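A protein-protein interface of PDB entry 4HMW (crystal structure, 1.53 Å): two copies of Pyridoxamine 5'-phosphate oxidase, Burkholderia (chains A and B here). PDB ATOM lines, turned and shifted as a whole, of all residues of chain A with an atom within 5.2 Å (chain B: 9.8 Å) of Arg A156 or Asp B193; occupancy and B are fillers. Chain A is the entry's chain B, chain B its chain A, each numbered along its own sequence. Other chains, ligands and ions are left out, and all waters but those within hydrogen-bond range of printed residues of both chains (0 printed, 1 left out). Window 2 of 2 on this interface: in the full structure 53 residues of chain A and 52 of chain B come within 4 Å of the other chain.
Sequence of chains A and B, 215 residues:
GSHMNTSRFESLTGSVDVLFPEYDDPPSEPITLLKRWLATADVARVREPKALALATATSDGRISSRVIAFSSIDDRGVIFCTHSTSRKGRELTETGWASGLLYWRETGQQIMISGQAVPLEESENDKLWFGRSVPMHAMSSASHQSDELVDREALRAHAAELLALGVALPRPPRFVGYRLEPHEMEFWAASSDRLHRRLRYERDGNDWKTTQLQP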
ATOM      1  N   MET A 139       5.638   5.873   5.407  1.00  0.00           N
ATOM      2  CA  MET A 139       4.469   5.187   5.929  1.00  0.00           C
ATOM      3  C   MET A 139       3.204   6.026   5.690  1.00  0.00           C
ATOM      4  O   MET A 139       2.139   5.487   5.352  1.00  0.00           O
ATOM      5  CB  MET A 139       4.627   4.864   7.429  1.00  0.00           C
ATOM      6  CG  MET A 139       3.455   4.039   8.010  1.00  0.00           C
ATOM      7  SD  MET A 139       3.207   2.488   7.131  1.00  0.00           S
ATOM      8  CE  MET A 139       4.675   1.573   7.619  1.00  0.00           C
ATOM      9  N   ARG A 152      -1.516  -6.193   4.911  1.00  0.00           N
ATOM     10  CA  ARG A 152      -0.559  -5.551   5.810  1.00  0.00           C
ATOM     11  C   ARG A 152       0.884  -5.643   5.288  1.00  0.00           C
ATOM     12  O   ARG A 152       1.632  -4.645   5.272  1.00  0.00           O
ATOM     13  CB  ARG A 152      -0.691  -6.171   7.210  1.00  0.00           C
ATOM     14  CG  ARG A 152       0.354  -5.730   8.213  1.00  0.00           C
ATOM     15  CD  ARG A 152      -0.029  -6.154   9.636  1.00  0.00           C
ATOM     16  NE  ARG A 152       0.963  -5.758  10.637  1.00  0.00           N
ATOM     17  CZ  ARG A 152       0.840  -4.740  11.501  1.00  0.00           C
ATOM     18  NH1 ARG A 152       1.818  -4.495  12.362  1.00  0.00           N
ATOM     19  NH2 ARG A 152      -0.244  -3.962  11.536  1.00  0.00           N
ATOM     20  N   GLU A 153       1.277  -6.823   4.825  1.00  0.00           N
ATOM     21  CA  GLU A 153       2.646  -6.989   4.331  1.00  0.00           C
ATOM     22  C   GLU A 153       2.903  -6.146   3.095  1.00  0.00           C
ATOM     23  O   GLU A 153       3.978  -5.596   2.944  1.00  0.00           O
ATOM     24  CB  GLU A 153       2.965  -8.460   4.050  1.00  0.00           C
ATOM     25  CG  GLU A 153       2.979  -9.335   5.310  1.00  0.00           C
ATOM     26  CD  GLU A 153       3.663  -8.675   6.513  1.00  0.00           C
ATOM     27  OE1 GLU A 153       4.750  -8.077   6.334  1.00  0.00           O
ATOM     28  OE2 GLU A 153       3.113  -8.755   7.642  1.00  0.00           O
ATOM     29  N   ALA A 154       1.909  -6.028   2.225  1.00  0.00           N
ATOM     30  CA  ALA A 154       2.016  -5.167   1.053  1.00  0.00           C
ATOM     31  C   ALA A 154       2.240  -3.721   1.458  1.00  0.00           C
ATOM     32  O   ALA A 154       3.082  -3.038   0.885  1.00  0.00           O
ATOM     33  CB  ALA A 154       0.756  -5.284   0.195  1.00  0.00           C
ATOM     34  N   LEU A 155       1.492  -3.252   2.453  1.00  0.00           N
ATOM     35  CA  LEU A 155       1.655  -1.890   2.938  1.00  0.00           C
ATOM     36  C   LEU A 155       3.077  -1.705   3.482  1.00  0.00           C
ATOM     37  O   LEU A 155       3.788  -0.764   3.119  1.00  0.00           O
ATOM     38  CB  LEU A 155       0.611  -1.609   4.033  1.00  0.00           C
ATOM     39  CG  LEU A 155       0.093  -0.170   4.116  1.00  0.00           C
ATOM     40  CD1 LEU A 155      -0.858  -0.014   5.293  1.00  0.00           C
ATOM     41  CD2 LEU A 155       1.220   0.795   4.220  1.00  0.00           C
ATOM     42  N   ARG A 156       3.507  -2.617   4.343  1.00  0.00           N
ATOM     43  CA  ARG A 156       4.859  -2.551   4.875  1.00  0.00           C
ATOM     44  C   ARG A 156       5.892  -2.504   3.752  1.00  0.00           C
ATOM     45  O   ARG A 156       6.811  -1.684   3.779  1.00  0.00           O
ATOM     46  CB  ARG A 156       5.114  -3.750   5.783  1.00  0.00           C
ATOM     47  CG  ARG A 156       6.414  -3.650   6.559  1.00  0.00           C
ATOM     48  CD  ARG A 156       6.539  -4.768   7.579  1.00  0.00           C
ATOM     49  NE  ARG A 156       5.744  -4.509   8.783  1.00  0.00           N
ATOM     50  CZ  ARG A 156       4.867  -5.352   9.331  1.00  0.00           C
ATOM     51  NH1 ARG A 156       4.635  -6.553   8.800  1.00  0.00           N
ATOM     52  NH2 ARG A 156       4.214  -4.992  10.422  1.00  0.00           N
ATOM     53  N   ALA A 157       5.716  -3.371   2.757  1.00  0.00           N
ATOM     54  CA  ALA A 157       6.655  -3.452   1.636  1.00  0.00           C
ATOM     55  C   ALA A 157       6.697  -2.168   0.814  1.00  0.00           C
ATOM     56  O   ALA A 157       7.770  -1.771   0.327  1.00  0.00           O
ATOM     57  CB  ALA A 157       6.308  -4.643   0.725  1.00  0.00           C
ATOM     58  N   HIS A 158       5.540  -1.533   0.618  1.00  0.00           N
ATOM     59  CA  HIS A 158       5.500  -0.312  -0.186  1.00  0.00           C
ATOM     60  C   HIS A 158       6.177   0.827   0.556  1.00  0.00           C
ATOM     61  O   HIS A 158       6.870   1.632  -0.041  1.00  0.00           O
ATOM     62  CB  HIS A 158       4.076   0.081  -0.572  1.00  0.00           C
ATOM     63  CG  HIS A 158       3.488  -0.808  -1.604  1.00  0.00           C
ATOM     64  ND1 HIS A 158       4.172  -1.155  -2.753  1.00  0.00           N
ATOM     65  CD2 HIS A 158       2.293  -1.449  -1.664  1.00  0.00           C
ATOM     66  CE1 HIS A 158       3.419  -1.956  -3.480  1.00  0.00           C
ATOM     67  NE2 HIS A 158       2.279  -2.155  -2.841  1.00  0.00           N
ATOM     68  N   ALA A 159       5.996   0.884   1.869  1.00  0.00           N
ATOM     69  CA  ALA A 159       6.682   1.913   2.645  1.00  0.00           C
ATOM     70  C   ALA A 159       8.187   1.745   2.536  1.00  0.00           C
ATOM     71  O   ALA A 159       8.909   2.728   2.368  1.00  0.00           O
ATOM     72  CB  ALA A 159       6.221   1.894   4.114  1.00  0.00           C
ATOM     73  N   ALA A 160       8.657   0.506   2.599  1.00  0.00           N
ATOM     74  CA  ALA A 160      10.080   0.217   2.455  1.00  0.00           C
ATOM     75  C   ALA A 160      10.624   0.634   1.077  1.00  0.00           C
ATOM     76  O   ALA A 160      11.730   1.175   0.971  1.00  0.00           O
ATOM     77  CB  ALA A 160      10.314  -1.260   2.672  1.00  0.00           C
ATOM     78  N   SER B  15       6.539   0.407  25.486  1.00  0.00           N
ATOM     79  CA  SER B  15       5.396   1.167  24.984  1.00  0.00           C
ATOM     80  C   SER B  15       5.126   0.915  23.503  1.00  0.00           C
ATOM     81  O   SER B  15       4.232   1.524  22.916  1.00  0.00           O
ATOM     82  CB  SER B  15       5.597   2.662  25.234  1.00  0.00           C
ATOM     83  OG  SER B  15       6.700   3.145  24.507  1.00  0.00           O
ATOM     84  N   VAL B  16       5.900   0.021  22.897  1.00  0.00           N
ATOM     85  CA  VAL B  16       5.690  -0.338  21.505  1.00  0.00           C
ATOM     86  C   VAL B  16       5.687  -1.856  21.349  1.00  0.00           C
ATOM     87  O   VAL B  16       6.320  -2.574  22.130  1.00  0.00           O
ATOM     88  CB  VAL B  16       6.772   0.273  20.612  1.00  0.00           C
ATOM     89  CG1 VAL B  16       6.677  -0.284  19.233  1.00  0.00           C
ATOM     90  CG2 VAL B  16       6.637   1.794  20.558  1.00  0.00           C
ATOM     91  N   ASP B  17       4.951  -2.338  20.352  1.00  0.00           N
ATOM     92  CA  ASP B  17       4.945  -3.750  19.994  1.00  0.00           C
ATOM     93  C   ASP B  17       4.430  -4.649  21.113  1.00  0.00           C
ATOM     94  O   ASP B  17       4.877  -5.778  21.247  1.00  0.00           O
ATOM     95  CB  ASP B  17       6.356  -4.180  19.566  1.00  0.00           C
ATOM     96  CG  ASP B  17       6.856  -3.397  18.355  1.00  0.00           C
ATOM     97  OD1 ASP B  17       6.020  -3.019  17.499  1.00  0.00           O
ATOM     98  OD2 ASP B  17       8.084  -3.131  18.266  1.00  0.00           O
ATOM     99  N   TYR B  23      -5.627  -9.145  17.315  1.00  0.00           N
ATOM    100  CA  TYR B  23      -5.644  -8.325  16.108  1.00  0.00           C
ATOM    101  C   TYR B  23      -6.050  -9.202  14.918  1.00  0.00           C
ATOM    102  O   TYR B  23      -6.850  -8.801  14.077  1.00  0.00           O
ATOM    103  CB  TYR B  23      -4.259  -7.712  15.918  1.00  0.00           C
ATOM    104  CG  TYR B  23      -4.022  -6.899  14.660  1.00  0.00           C
ATOM    105  CD1 TYR B  23      -4.757  -5.744  14.390  1.00  0.00           C
ATOM    106  CD2 TYR B  23      -3.011  -7.248  13.789  1.00  0.00           C
ATOM    107  CE1 TYR B  23      -4.496  -4.981  13.244  1.00  0.00           C
ATOM    108  CE2 TYR B  23      -2.749  -6.508  12.670  1.00  0.00           C
ATOM    109  CZ  TYR B  23      -3.482  -5.373  12.405  1.00  0.00           C
ATOM    110  OH  TYR B  23      -3.201  -4.644  11.271  1.00  0.00           O
ATOM    111  N   ASP B  24      -5.520 -10.417  14.884  1.00  0.00           N
ATOM    112  CA  ASP B  24      -5.824 -11.373  13.810  1.00  0.00           C
ATOM    113  C   ASP B  24      -6.896 -12.395  14.175  1.00  0.00           C
ATOM    114  O   ASP B  24      -7.407 -13.078  13.297  1.00  0.00           O
ATOM    115  CB  ASP B  24      -4.558 -12.096  13.397  1.00  0.00           C
ATOM    116  CG  ASP B  24      -3.594 -11.184  12.664  1.00  0.00           C
ATOM    117  OD1 ASP B  24      -4.046 -10.473  11.738  1.00  0.00           O
ATOM    118  OD2 ASP B  24      -2.399 -11.155  13.033  1.00  0.00           O
ATOM    119  N   ALA B 189      -2.777  -0.334  19.025  1.00  0.00           N
ATOM    120  CA  ALA B 189      -1.539  -0.692  19.701  1.00  0.00           C
ATOM    121  C   ALA B 189      -0.368  -0.252  18.840  1.00  0.00           C
ATOM    122  O   ALA B 189      -0.271  -0.632  17.656  1.00  0.00           O
ATOM    123  CB  ALA B 189      -1.477  -2.184  19.979  1.00  0.00           C
ATOM    124  N   ALA B 190       0.518   0.548  19.437  1.00  0.00           N
ATOM    125  CA  ALA B 190       1.633   1.144  18.707  1.00  0.00           C
ATOM    126  C   ALA B 190       2.620   0.085  18.242  1.00  0.00           C
ATOM    127  O   ALA B 190       2.859  -0.905  18.937  1.00  0.00           O
ATOM    128  CB  ALA B 190       2.356   2.155  19.565  1.00  0.00           C
ATOM    129  N   SER B 191       3.270   0.402  17.124  1.00  0.00           N
ATOM    130  CA  SER B 191       4.231  -0.474  16.477  1.00  0.00           C
ATOM    131  C   SER B 191       5.477   0.335  16.161  1.00  0.00           C
ATOM    132  O   SER B 191       5.393   1.465  15.676  1.00  0.00           O
ATOM    133  CB  SER B 191       3.649  -1.077  15.196  1.00  0.00           C
ATOM    134  OG  SER B 191       2.724  -2.100  15.505  1.00  0.00           O
ATOM    135  N   SER B 192       6.641  -0.246  16.445  1.00  0.00           N
ATOM    136  CA  SER B 192       7.900   0.455  16.256  1.00  0.00           C
ATOM    137  C   SER B 192       8.147   0.794  14.785  1.00  0.00           C
ATOM    138  O   SER B 192       8.844   1.765  14.488  1.00  0.00           O
ATOM    139  CB  SER B 192       9.055  -0.390  16.795  1.00  0.00           C
ATOM    140  OG  SER B 192       8.993  -1.692  16.240  1.00  0.00           O
ATOM    141  N   ASP B 193       7.575   0.007  13.872  1.00  0.00           N
ATOM    142  CA  ASP B 193       7.683   0.296  12.427  1.00  0.00           C
ATOM    143  C   ASP B 193       6.594   1.233  11.871  1.00  0.00           C
ATOM    144  O   ASP B 193       6.482   1.405  10.648  1.00  0.00           O
ATOM    145  CB  ASP B 193       7.736  -0.995  11.602  1.00  0.00           C
ATOM    146  CG  ASP B 193       6.429  -1.785  11.614  1.00  0.00           C
ATOM    147  OD1 ASP B 193       5.413  -1.360  12.220  1.00  0.00           O
ATOM    148  OD2 ASP B 193       6.417  -2.865  10.982  1.00  0.00           O
ATOM    149  N   ARG B 194       5.816   1.828  12.775  1.00  0.00           N
ATOM    150  CA  ARG B 194       4.746   2.778  12.441  1.00  0.00           C
ATOM    151  C   ARG B 194       3.490   2.165  11.829  1.00  0.00           C
ATOM    152  O   ARG B 194       2.520   2.884  11.583  1.00  0.00           O
ATOM    153  CB  ARG B 194       5.259   3.872  11.512  1.00  0.00           C
ATOM    154  CG  ARG B 194       6.363   4.708  12.108  1.00  0.00           C
ATOM    155  CD  ARG B 194       6.971   5.563  11.002  1.00  0.00           C
ATOM    156  NE  ARG B 194       8.251   6.123  11.406  1.00  0.00           N
ATOM    157  CZ  ARG B 194       8.396   7.294  12.015  1.00  0.00           C
ATOM    158  NH1 ARG B 194       7.334   8.058  12.278  1.00  0.00           N
ATOM    159  NH2 ARG B 194       9.615   7.701  12.356  1.00  0.00           N
ATOM    160  N   LEU B 195       3.513   0.864  11.551  1.00  0.00           N
ATOM    161  CA  LEU B 195       2.313   0.183  11.076  1.00  0.00           C
ATOM    162  C   LEU B 195       1.482  -0.294  12.280  1.00  0.00           C
ATOM    163  O   LEU B 195       1.440  -1.472  12.622  1.00  0.00           O
ATOM    164  CB  LEU B 195       2.682  -0.964  10.132  1.00  0.00           C
ATOM    165  CG  LEU B 195       1.711  -1.091   8.944  1.00  0.00           C
ATOM    166  CD1 LEU B 195       2.211  -2.090   7.905  1.00  0.00           C
ATOM    167  CD2 LEU B 195       0.325  -1.485   9.423  1.00  0.00           C
ATOM    168  N   HIS B 196       0.810   0.649  12.908  1.00  0.00           N
ATOM    169  CA  HIS B 196       0.070   0.359  14.130  1.00  0.00           C
ATOM    170  C   HIS B 196      -1.034  -0.670  13.916  1.00  0.00           C
ATOM    171  O   HIS B 196      -1.642  -0.726  12.866  1.00  0.00           O
ATOM    172  CB  HIS B 196      -0.516   1.661  14.685  1.00  0.00           C
ATOM    173  CG  HIS B 196       0.505   2.743  14.814  1.00  0.00           C
ATOM    174  ND1 HIS B 196       1.705   2.525  15.445  1.00  0.00           N
ATOM    175  CD2 HIS B 196       0.530   4.029  14.388  1.00  0.00           C
ATOM    176  CE1 HIS B 196       2.433   3.625  15.407  1.00  0.00           C
ATOM    177  NE2 HIS B 196       1.740   4.558  14.777  1.00  0.00           N
ATOM    178  N   ARG B 197      -1.297  -1.461  14.943  1.00  0.00           N
ATOM    179  CA  ARG B 197      -2.351  -2.452  14.920  1.00  0.00           C
ATOM    180  C   ARG B 197      -3.650  -1.744  15.307  1.00  0.00           C
ATOM    181  O   ARG B 197      -3.757  -1.213  16.408  1.00  0.00           O
ATOM    182  CB  ARG B 197      -2.054  -3.564  15.929  1.00  0.00           C
ATOM    183  CG  ARG B 197      -1.034  -4.630  15.494  1.00  0.00           C
ATOM    184  CD  ARG B 197       0.418  -4.231  15.693  1.00  0.00           C
ATOM    185  NE  ARG B 197       0.779  -3.613  16.993  1.00  0.00           N
ATOM    186  CZ  ARG B 197       1.148  -4.279  18.093  1.00  0.00           C
ATOM    187  NH1 ARG B 197       1.159  -5.604  18.122  1.00  0.00           N
ATOM    188  NH2 ARG B 197       1.495  -3.624  19.189  1.00  0.00           N
ATOM    189  N   GLN B 214      -5.937   0.843   8.362  1.00  0.00           N
ATOM    190  CA  GLN B 214      -4.637   1.426   8.041  1.00  0.00           C
ATOM    191  C   GLN B 214      -4.288   2.531   9.041  1.00  0.00           C
ATOM    192  O   GLN B 214      -5.165   3.289   9.470  1.00  0.00           O
ATOM    193  CB  GLN B 214      -4.661   1.974   6.621  1.00  0.00           C
ATOM    194  CG  GLN B 214      -4.941   0.883   5.587  1.00  0.00           C
ATOM    195  CD  GLN B 214      -4.846   1.418   4.163  1.00  0.00           C
ATOM    196  OE1 GLN B 214      -3.868   2.073   3.799  1.00  0.00           O
ATOM    197  NE2 GLN B 214      -5.859   1.130   3.355  1.00  0.00           N
ATOM    198  N   PRO B 215      -2.996   2.640   9.380  1.00  0.00           N
ATOM    199  CA  PRO B 215      -2.519   3.513  10.463  1.00  0.00           C
ATOM    200  C   PRO B 215      -2.453   5.002  10.112  1.00  0.00           C
ATOM    201  O   PRO B 215      -2.354   5.382   8.932  1.00  0.00           O
ATOM    202  CB  PRO B 215      -1.108   2.979  10.742  1.00  0.00           C
ATOM    203  CG  PRO B 215      -0.650   2.440   9.390  1.00  0.00           C
ATOM    204  CD  PRO B 215      -1.915   1.820   8.805  1.00  0.00           C
ATOM    205  OXT PRO B 215      -2.481   5.850  11.054  1.00  0.00           O
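Met A139 touches Asp B193.
CG of Met A139 touches O of Arg B194 (3.9 Å).
Arg A152 touches His B196 (NH2 to O, 3.8 Å).
Arg A152 touches Arg B197.
Leu A155 touches Gln B214 (CD1 to OE1, 3.96 Å).
N of Arg A156 touches CD1 of Leu B195, at 3.8 Å.
The backbone NH (N) of Ala B189 is in hydrogen-bond range of the backbone carbonyl oxygen (O) of Arg B197 (2.9 Å).
O of Ala B190 lies within hydrogen-bond range of NH2 of Arg B197, at 3.1 Å.
OG of Ser B191 is in hydrogen-bond range of O of Leu B195 (3.2 Å).
The backbone NH (N) of Ser B191 sits at hydrogen-bond distance from a ring nitrogen (ND1) of His B196, 3.1 Å away.
The side-chain carboxylate (OD1) of Asp B193 is in hydrogen-bond range of the backbone NH (N) of Leu B195 (3.0 Å).
The guanidinium group of Arg A156 is in salt-bridge range of the side-chain carboxylate of Glu A153 (2.9 Å).
Asp B193 touches two residues of chain A.
No residue of chain B comes within 4 Å of Glu A153.
Of the printed residues of chain B, Leu A155 touches Gln B214 (3.96 Å).
No residue of chain B comes within 4 Å of Ala A157.
Ala A159 touches none of the printed residues of chain B.
Of the printed residues of chain A, Gln B214 touches Leu A155 (3.96 Å).
Printed residues of chain A within 4 Å of Arg B197: Arg A152.
Of the printed residues of chain A, Arg B194 touches Met A139 (3.9 Å).
Asp B17 touches none of the printed residues of chain A.
Ser B192 touches none of the printed residues of chain A.
The nearest residue of chain A that does not touch Asp B193 is Arg A152 (4.8 Å).
Of the 16 printed residues of chain B, 7 touch a printed residue of chain A.
Hydrophobic or aromatic side chains of chain B within 4 Å of the printed part of chain A: Tyr B23 and Leu B195.
Along chain A the printed residues that touch a printed residue of chain B span positions 139 to 156.
Among the printed residues, 9 pairs touch across the chains.
Among the printed residues, Asp or Glu carboxylates within 4 Å of a Lys or Arg side-chain nitrogen of the other chain: Arg A156 with Asp B193 (2.8 Å).
The side-chain hydroxyl (OH) of Tyr B23 sits at hydrogen-bond distance from the guanidinium group (NH2) of Arg A152 (3.0 Å).
The guanidinium group (NE) of Arg A156 is in salt-bridge range of the side-chain carboxylate (OD2) of Asp B193, 2.8 Å away.
O of Leu B195 is in hydrogen-bond range of NH1 of Arg A152, at 3.1 Å.
No position is printed for both chains.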
